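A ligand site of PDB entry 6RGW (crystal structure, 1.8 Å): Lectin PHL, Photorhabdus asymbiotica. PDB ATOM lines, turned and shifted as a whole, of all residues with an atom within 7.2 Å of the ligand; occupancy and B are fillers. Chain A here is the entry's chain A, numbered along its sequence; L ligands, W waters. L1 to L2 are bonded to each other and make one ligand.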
ATOM      1  N   ASP A  51       4.308 -17.365 -28.218  1.00  0.00           N
ATOM      2  CA  ASP A  51       5.668 -17.965 -28.271  1.00  0.00           C
ATOM      3  C   ASP A  51       5.617 -19.362 -28.912  1.00  0.00           C
ATOM      4  O   ASP A  51       6.691 -19.968 -29.037  1.00  0.00           O
ATOM      5  CB  ASP A  51       6.298 -18.005 -26.875  1.00  0.00           C
ATOM      6  CG  ASP A  51       5.541 -18.810 -25.816  1.00  0.00           C
ATOM      7  OD1 ASP A  51       4.325 -19.082 -26.032  1.00  0.00           O
ATOM      8  OD2 ASP A  51       6.162 -19.140 -24.770  1.00  0.00           O
ATOM      9  N   LYS A  52       4.426 -19.841 -29.305  1.00  0.00           N
ATOM     10  CA  LYS A  52       4.200 -21.160 -29.961  1.00  0.00           C
ATOM     11  C   LYS A  52       4.450 -22.311 -28.961  1.00  0.00           C
ATOM     12  O   LYS A  52       4.502 -23.470 -29.418  1.00  0.00           O
ATOM     13  CB  LYS A  52       5.065 -21.322 -31.213  1.00  0.00           C
ATOM     14  CG  LYS A  52       4.792 -20.275 -32.283  1.00  0.00           C
ATOM     15  CD  LYS A  52       5.238 -20.679 -33.671  1.00  0.00           C
ATOM     16  CE  LYS A  52       5.063 -19.544 -34.657  1.00  0.00           C
ATOM     17  NZ  LYS A  52       5.587 -19.880 -35.998  1.00  0.00           N
ATOM     18  N   ALA A  53       4.548 -22.009 -27.658  1.00  0.00           N
ATOM     19  CA  ALA A  53       4.592 -23.053 -26.607  1.00  0.00           C
ATOM     20  C   ALA A  53       3.160 -23.477 -26.261  1.00  0.00           C
ATOM     21  O   ALA A  53       2.219 -22.717 -26.536  1.00  0.00           O
ATOM     22  CB  ALA A  53       5.316 -22.554 -25.378  1.00  0.00           C
ATOM     23  N   VAL A  54       3.015 -24.674 -25.711  1.00  0.00           N
ATOM     24  CA  VAL A  54       1.721 -25.170 -25.185  1.00  0.00           C
ATOM     25  C   VAL A  54       1.632 -24.702 -23.739  1.00  0.00           C
ATOM     26  O   VAL A  54       2.604 -24.916 -22.996  1.00  0.00           O
ATOM     27  CB  VAL A  54       1.597 -26.701 -25.319  1.00  0.00           C
ATOM     28  CG1 VAL A  54       0.294 -27.196 -24.715  1.00  0.00           C
ATOM     29  CG2 VAL A  54       1.727 -27.151 -26.769  1.00  0.00           C
ATOM     30  N   SER A  73       3.455 -22.875 -18.716  1.00  0.00           N
ATOM     31  CA  SER A  73       3.984 -23.370 -20.011  1.00  0.00           C
ATOM     32  C   SER A  73       4.449 -24.818 -19.876  1.00  0.00           C
ATOM     33  O   SER A  73       5.153 -25.150 -18.894  1.00  0.00           O
ATOM     34  CB  SER A  73       5.096 -22.481 -20.495  1.00  0.00           C
ATOM     35  OG  SER A  73       5.635 -23.011 -21.698  1.00  0.00           O
ATOM     36  N   LEU A  74       4.081 -25.659 -20.836  1.00  0.00           N
ATOM     37  CA  LEU A  74       4.672 -27.008 -21.037  1.00  0.00           C
ATOM     38  C   LEU A  74       5.796 -26.899 -22.069  1.00  0.00           C
ATOM     39  O   LEU A  74       6.389 -27.939 -22.409  1.00  0.00           O
ATOM     40  CB  LEU A  74       3.588 -27.976 -21.521  1.00  0.00           C
ATOM     41  CG  LEU A  74       2.463 -28.261 -20.527  1.00  0.00           C
ATOM     42  CD1 LEU A  74       1.452 -29.228 -21.136  1.00  0.00           C
ATOM     43  CD2 LEU A  74       3.003 -28.809 -19.221  1.00  0.00           C
ATOM     44  N   LYS A  75       6.087 -25.679 -22.546  1.00  0.00           N
ATOM     45  CA  LYS A  75       7.136 -25.406 -23.564  1.00  0.00           C
ATOM     46  C   LYS A  75       6.745 -26.090 -24.874  1.00  0.00           C
ATOM     47  O   LYS A  75       5.533 -26.165 -25.159  1.00  0.00           O
ATOM     48  CB  LYS A  75       8.509 -25.853 -23.038  1.00  0.00           C
ATOM     49  CG  LYS A  75       8.936 -25.231 -21.712  1.00  0.00           C
ATOM     50  CD  LYS A  75      10.181 -25.878 -21.143  1.00  0.00           C
ATOM     51  CE  LYS A  75      11.004 -24.946 -20.280  1.00  0.00           C
ATOM     52  NZ  LYS A  75      12.222 -25.612 -19.767  1.00  0.00           N
ATOM     53  N   GLY A  76       7.724 -26.560 -25.645  1.00  0.00           N
ATOM     54  CA  GLY A  76       7.515 -27.052 -27.019  1.00  0.00           C
ATOM     55  C   GLY A  76       7.338 -25.898 -27.983  1.00  0.00           C
ATOM     56  O   GLY A  76       7.236 -24.742 -27.538  1.00  0.00           O
ATOM     57  N   GLN A  77       7.335 -26.206 -29.280  1.00  0.00           N
ATOM     58  CA  GLN A  77       7.086 -25.234 -30.372  1.00  0.00           C
ATOM     59  C   GLN A  77       6.171 -25.959 -31.352  1.00  0.00           C
ATOM     60  O   GLN A  77       6.636 -26.927 -31.984  1.00  0.00           O
ATOM     61  CB  GLN A  77       8.411 -24.778 -31.008  1.00  0.00           C
ATOM     62  CG  GLN A  77       9.263 -23.927 -30.074  1.00  0.00           C
ATOM     63  CD  GLN A  77       8.701 -22.539 -29.883  1.00  0.00           C
ATOM     64  OE1 GLN A  77       8.921 -21.650 -30.709  1.00  0.00           O
ATOM     65  NE2 GLN A  77       7.992 -22.331 -28.786  1.00  0.00           N
ATOM     66  N   VAL A  78       4.895 -25.566 -31.403  1.00  0.00           N
ATOM     67  CA  VAL A  78       3.833 -26.355 -32.071  1.00  0.00           C
ATOM     68  C   VAL A  78       3.205 -25.542 -33.205  1.00  0.00           C
ATOM     69  O   VAL A  78       3.133 -24.290 -33.091  1.00  0.00           O
ATOM     70  CB  VAL A  78       2.764 -26.848 -31.075  1.00  0.00           C
ATOM     71  CG1 VAL A  78       3.389 -27.680 -29.972  1.00  0.00           C
ATOM     72  CG2 VAL A  78       1.934 -25.719 -30.489  1.00  0.00           C
ATOM     73  N   THR A  79       2.717 -26.255 -34.221  1.00  0.00           N
ATOM     74  CA  THR A  79       2.039 -25.720 -35.432  1.00  0.00           C
ATOM     75  C   THR A  79       0.693 -26.431 -35.644  1.00  0.00           C
ATOM     76  O   THR A  79       0.202 -26.459 -36.796  1.00  0.00           O
ATOM     77  CB  THR A  79       2.981 -25.836 -36.626  1.00  0.00           C
ATOM     78  OG1 THR A  79       3.275 -27.226 -36.821  1.00  0.00           O
ATOM     79  CG2 THR A  79       4.269 -25.071 -36.432  1.00  0.00           C
ATOM     80  N   ALA A  96       0.604 -32.808 -30.459  1.00  0.00           N
ATOM     81  CA  ALA A  96       0.693 -31.584 -31.266  1.00  0.00           C
ATOM     82  C   ALA A  96       1.659 -31.800 -32.430  1.00  0.00           C
ATOM     83  O   ALA A  96       2.652 -32.534 -32.250  1.00  0.00           O
ATOM     84  CB  ALA A  96       1.137 -30.429 -30.410  1.00  0.00           C
ATOM     85  N   ARG A  97       1.397 -31.133 -33.550  1.00  0.00           N
ATOM     86  CA  ARG A  97       2.400 -31.010 -34.631  1.00  0.00           C
ATOM     87  C   ARG A  97       3.485 -30.047 -34.169  1.00  0.00           C
ATOM     88  O   ARG A  97       3.129 -28.979 -33.618  1.00  0.00           O
ATOM     89  CB  ARG A  97       1.775 -30.526 -35.938  1.00  0.00           C
ATOM     90  CG  ARG A  97       2.732 -30.607 -37.105  1.00  0.00           C
ATOM     91  CD  ARG A  97       2.073 -30.227 -38.413  1.00  0.00           C
ATOM     92  NE  ARG A  97       1.695 -28.820 -38.454  1.00  0.00           N
ATOM     93  CZ  ARG A  97       1.227 -28.204 -39.528  1.00  0.00           C
ATOM     94  NH1 ARG A  97       1.090 -28.869 -40.667  1.00  0.00           N
ATOM     95  NH2 ARG A  97       0.900 -26.927 -39.475  1.00  0.00           N
ATOM     96  N   GLY A  98       4.750 -30.418 -34.360  1.00  0.00           N
ATOM     97  CA  GLY A  98       5.919 -29.578 -34.074  1.00  0.00           C
ATOM     98  C   GLY A  98       6.190 -28.653 -35.252  1.00  0.00           C
ATOM     99  O   GLY A  98       5.600 -28.852 -36.318  1.00  0.00           O
ATOM    100  N   THR A  99       7.032 -27.637 -35.048  1.00  0.00           N
ATOM    101  CA  THR A  99       7.527 -26.741 -36.130  1.00  0.00           C
ATOM    102  C   THR A  99       8.244 -27.577 -37.199  1.00  0.00           C
ATOM    103  O   THR A  99       8.334 -27.069 -38.342  1.00  0.00           O
ATOM    104  CB  THR A  99       8.374 -25.603 -35.538  1.00  0.00           C
ATOM    105  OG1 THR A  99       9.348 -26.168 -34.658  1.00  0.00           O
ATOM    106  CG2 THR A  99       7.551 -24.577 -34.787  1.00  0.00           C
ATOM    107  N   ASP A 100       8.698 -28.790 -36.880  1.00  0.00           N
ATOM    108  CA  ASP A 100       9.343 -29.724 -37.849  1.00  0.00           C
ATOM    109  C   ASP A 100       8.299 -30.585 -38.591  1.00  0.00           C
ATOM    110  O   ASP A 100       8.718 -31.453 -39.374  1.00  0.00           O
ATOM    111  CB  ASP A 100      10.404 -30.601 -37.174  1.00  0.00           C
ATOM    112  CG  ASP A 100       9.857 -31.589 -36.161  1.00  0.00           C
ATOM    113  OD1 ASP A 100       8.629 -31.540 -35.910  1.00  0.00           O
ATOM    114  OD2 ASP A 100      10.649 -32.393 -35.648  1.00  0.00           O
ATOM    115  N   ASN A 101       7.005 -30.356 -38.340  1.00  0.00           N
ATOM    116  CA  ASN A 101       5.848 -31.050 -38.969  1.00  0.00           C
ATOM    117  C   ASN A 101       5.743 -32.521 -38.518  1.00  0.00           C
ATOM    118  O   ASN A 101       4.878 -33.237 -39.067  1.00  0.00           O
ATOM    119  CB  ASN A 101       5.884 -30.933 -40.491  1.00  0.00           C
ATOM    120  CG  ASN A 101       5.564 -29.536 -40.940  1.00  0.00           C
ATOM    121  OD1 ASN A 101       4.567 -28.959 -40.503  1.00  0.00           O
ATOM    122  ND2 ASN A 101       6.415 -28.965 -41.786  1.00  0.00           N
ATOM    123  N   ALA A 102       6.537 -32.966 -37.554  1.00  0.00           N
ATOM    124  CA  ALA A 102       6.364 -34.305 -36.944  1.00  0.00           C
ATOM    125  C   ALA A 102       5.245 -34.250 -35.909  1.00  0.00           C
ATOM    126  O   ALA A 102       4.829 -33.143 -35.484  1.00  0.00           O
ATOM    127  CB  ALA A 102       7.650 -34.813 -36.365  1.00  0.00           C
ATOM    128  N   LEU A 103       4.736 -35.419 -35.527  1.00  0.00           N
ATOM    129  CA  LEU A 103       3.842 -35.553 -34.360  1.00  0.00           C
ATOM    130  C   LEU A 103       4.728 -35.610 -33.117  1.00  0.00           C
ATOM    131  O   LEU A 103       5.647 -36.449 -33.062  1.00  0.00           O
ATOM    132  CB  LEU A 103       2.974 -36.811 -34.487  1.00  0.00           C
ATOM    133  CG  LEU A 103       2.139 -37.123 -33.242  1.00  0.00           C
ATOM    134  CD1 LEU A 103       1.085 -36.059 -33.023  1.00  0.00           C
ATOM    135  CD2 LEU A 103       1.503 -38.503 -33.356  1.00  0.00           C
ATOM    136  N   TRP A 104       4.430 -34.736 -32.156  1.00  0.00           N
ATOM    137  CA  TRP A 104       5.118 -34.701 -30.844  1.00  0.00           C
ATOM    138  C   TRP A 104       4.096 -35.027 -29.753  1.00  0.00           C
ATOM    139  O   TRP A 104       2.895 -34.793 -29.956  1.00  0.00           O
ATOM    140  CB  TRP A 104       5.758 -33.330 -30.604  1.00  0.00           C
ATOM    141  CG  TRP A 104       6.978 -33.090 -31.442  1.00  0.00           C
ATOM    142  CD1 TRP A 104       7.009 -32.788 -32.763  1.00  0.00           C
ATOM    143  CD2 TRP A 104       8.341 -33.154 -31.006  1.00  0.00           C
ATOM    144  NE1 TRP A 104       8.302 -32.649 -33.183  1.00  0.00           N
ATOM    145  CE2 TRP A 104       9.147 -32.867 -32.134  1.00  0.00           C
ATOM    146  CE3 TRP A 104       8.976 -33.410 -29.780  1.00  0.00           C
ATOM    147  CZ2 TRP A 104      10.542 -32.832 -32.060  1.00  0.00           C
ATOM    148  CZ3 TRP A 104      10.354 -33.376 -29.711  1.00  0.00           C
ATOM    149  CH2 TRP A 104      11.124 -33.086 -30.835  1.00  0.00           C
ATOM    150  N   HIS A 105       4.573 -35.505 -28.613  1.00  0.00           N
ATOM    151  CA  HIS A 105       3.680 -35.716 -27.449  1.00  0.00           C
ATOM    152  C   HIS A 105       4.454 -35.495 -26.153  1.00  0.00           C
ATOM    153  O   HIS A 105       5.692 -35.518 -26.171  1.00  0.00           O
ATOM    154  CB  HIS A 105       2.972 -37.076 -27.545  1.00  0.00           C
ATOM    155  CG  HIS A 105       3.855 -38.260 -27.391  1.00  0.00           C
ATOM    156  ND1 HIS A 105       3.469 -39.370 -26.669  1.00  0.00           N
ATOM    157  CD2 HIS A 105       5.097 -38.528 -27.849  1.00  0.00           C
ATOM    158  CE1 HIS A 105       4.425 -40.271 -26.695  1.00  0.00           C
ATOM    159  NE2 HIS A 105       5.446 -39.773 -27.416  1.00  0.00           N
ATOM    160  N   ASN A 117       9.357 -34.948 -20.735  1.00  0.00           N
ATOM    161  CA  ASN A 117       9.825 -34.013 -21.795  1.00  0.00           C
ATOM    162  C   ASN A 117       9.026 -34.324 -23.063  1.00  0.00           C
ATOM    163  O   ASN A 117       8.484 -35.454 -23.172  1.00  0.00           O
ATOM    164  CB  ASN A 117      11.327 -34.097 -22.014  1.00  0.00           C
ATOM    165  CG  ASN A 117      12.101 -33.570 -20.825  1.00  0.00           C
ATOM    166  OD1 ASN A 117      11.884 -32.445 -20.390  1.00  0.00           O
ATOM    167  ND2 ASN A 117      12.976 -34.390 -20.280  1.00  0.00           N
ATOM    168  N   TRP A 118       8.934 -33.344 -23.958  1.00  0.00           N
ATOM    169  CA  TRP A 118       8.378 -33.556 -25.317  1.00  0.00           C
ATOM    170  C   TRP A 118       9.207 -34.635 -26.008  1.00  0.00           C
ATOM    171  O   TRP A 118      10.444 -34.618 -25.874  1.00  0.00           O
ATOM    172  CB  TRP A 118       8.386 -32.254 -26.111  1.00  0.00           C
ATOM    173  CG  TRP A 118       7.310 -31.296 -25.726  1.00  0.00           C
ATOM    174  CD1 TRP A 118       7.399 -30.222 -24.886  1.00  0.00           C
ATOM    175  CD2 TRP A 118       5.954 -31.313 -26.211  1.00  0.00           C
ATOM    176  NE1 TRP A 118       6.202 -29.566 -24.829  1.00  0.00           N
ATOM    177  CE2 TRP A 118       5.292 -30.219 -25.616  1.00  0.00           C
ATOM    178  CE3 TRP A 118       5.232 -32.144 -27.076  1.00  0.00           C
ATOM    179  CZ2 TRP A 118       3.957 -29.937 -25.873  1.00  0.00           C
ATOM    180  CZ3 TRP A 118       3.908 -31.868 -27.327  1.00  0.00           C
ATOM    181  CH2 TRP A 118       3.289 -30.770 -26.738  1.00  0.00           C
ATOM    182  N   GLN A 119       8.543 -35.565 -26.695  1.00  0.00           N
ATOM    183  CA  GLN A 119       9.188 -36.633 -27.486  1.00  0.00           C
ATOM    184  C   GLN A 119       8.529 -36.645 -28.873  1.00  0.00           C
ATOM    185  O   GLN A 119       7.320 -36.414 -28.956  1.00  0.00           O
ATOM    186  CB  GLN A 119       9.078 -37.976 -26.751  1.00  0.00           C
ATOM    187  CG  GLN A 119       9.557 -39.178 -27.558  1.00  0.00           C
ATOM    188  CD  GLN A 119       9.086 -40.498 -27.003  1.00  0.00           C
ATOM    189  OE1 GLN A 119       8.068 -41.051 -27.423  1.00  0.00           O
ATOM    190  NE2 GLN A 119       9.840 -41.016 -26.047  1.00  0.00           N
HETATM  191  C1  LIG L   1      11.502 -27.872 -30.305  1.00  0.00           C
HETATM  192  C2  LIG L   1      12.363 -28.398 -31.440  1.00  0.00           C
HETATM  193  O1  LIG L   1      13.554 -27.619 -31.573  1.00  0.00           O
HETATM  194  O2  LIG L   1      10.364 -28.717 -30.174  1.00  0.00           O
HETATM  195  C3  LIG L   1       9.496 -28.645 -31.305  1.00  0.00           C
HETATM  196  C4  LIG L   1      10.237 -29.101 -32.573  1.00  0.00           C
HETATM  197  O3  LIG L   1       9.428 -28.915 -33.735  1.00  0.00           O
HETATM  198  C5  LIG L   1      11.555 -28.324 -32.734  1.00  0.00           C
HETATM  199  O4  LIG L   1      12.340 -28.840 -33.806  1.00  0.00           O
HETATM  200  C6  LIG L   1       8.277 -29.510 -30.993  1.00  0.00           C
HETATM  201  O5  LIG L   1       7.618 -28.989 -29.830  1.00  0.00           O
HETATM  202  C7  LIG L   1      12.580 -27.864 -34.830  1.00  0.00           C
HETATM  203  C8  LIG L   1       6.616 -29.868 -29.334  1.00  0.00           C
HETATM  204  C1  LG2 L   2      11.943 -26.906 -25.132  1.00  0.00           C
HETATM  205  C2  LG2 L   2      11.783 -25.794 -26.168  1.00  0.00           C
HETATM  206  C3  LG2 L   2      12.245 -26.275 -27.555  1.00  0.00           C
HETATM  207  C4  LG2 L   2      11.574 -27.591 -27.920  1.00  0.00           C
HETATM  208  C5  LG2 L   2      11.730 -28.624 -26.794  1.00  0.00           C
HETATM  209  C6  LG2 L   2      11.010 -29.918 -27.119  1.00  0.00           C
HETATM  210  O1  LG2 L   2      10.394 -25.407 -26.176  1.00  0.00           O
HETATM  211  O2  LG2 L   2      11.977 -25.290 -28.553  1.00  0.00           O
HETATM  212  O3  LG2 L   2      12.145 -28.145 -29.126  1.00  0.00           O
HETATM  213  O4  LG2 L   2      11.223 -28.072 -25.560  1.00  0.00           O
HETATM  214  C7  LG2 L   2      10.120 -24.002 -26.063  1.00  0.00           C
HETATM  215  C8  LG2 L   2      12.632 -24.028 -28.344  1.00  0.00           C
HETATM  216  O5  LG2 L   2      13.329 -27.220 -24.950  1.00  0.00           O
HETATM  217  O   HOH W   1      14.162 -31.699 -33.002  1.00  0.00           O
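O3 of LIG L1 is in hydrogen-bond range of OG1 of Thr 99. The backbone NH of Thr 99 lies within hydrogen-bond range of an oxygen (O3) of LIG L1. The backbone NH (N) of Asp 100 lies within hydrogen-bond range of an oxygen (O3) of LIG L1. An oxygen (O5) of LIG L1 is in hydrogen-bond range of the backbone NH (N) of Gln 77 (2.9 Å). The backbone NH (N) of Gly 76 sits at hydrogen-bond distance from an oxygen (O1) of LG2 L2, at 3.0 Å.
NE1 of Trp 118 is in hydrogen-bond range of O of Lys 75 (3.5 Å). N of Trp 104 lies within hydrogen-bond range of O of Ala 96, 2.8 Å away. The backbone NH of Ala 102 is in hydrogen-bond range of the side-chain carboxylate of Asp 100, at 3.0 Å. The backbone NH (N) of Val 54 is in hydrogen-bond range of the backbone carbonyl oxygen (O) of Lys 75 (3.0 Å). The indole nitrogen of Trp 104 is in hydrogen-bond range of the side-chain carboxylate of Asp 100, 3.0 Å away. The backbone carbonyl oxygen of Leu 74 lies within hydrogen-bond range of the indole nitrogen of Trp 118. The backbone carbonyl oxygen (O) of Lys 52 lies within hydrogen-bond range of the backbone NH (N) of Val 78 (2.9 Å). The backbone carbonyl oxygen (O) of Gln 77 lies within hydrogen-bond range of the backbone NH (N) of Thr 99, 3.2 Å away.
CB of Lys 75 touches O1 of LG2 L2 (3.7 Å). CG1 of Val 78 touches C8 of LIG L1, 3.95 Å away. Gly 98 touches the ligand. CD2 of Trp 104 touches C6 of LIG L1 (3.6 Å). Trp 118 touches the ligand. Hydrophobic or aromatic side chains that line the ligand: Val 78, Trp 104 and Trp 118.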
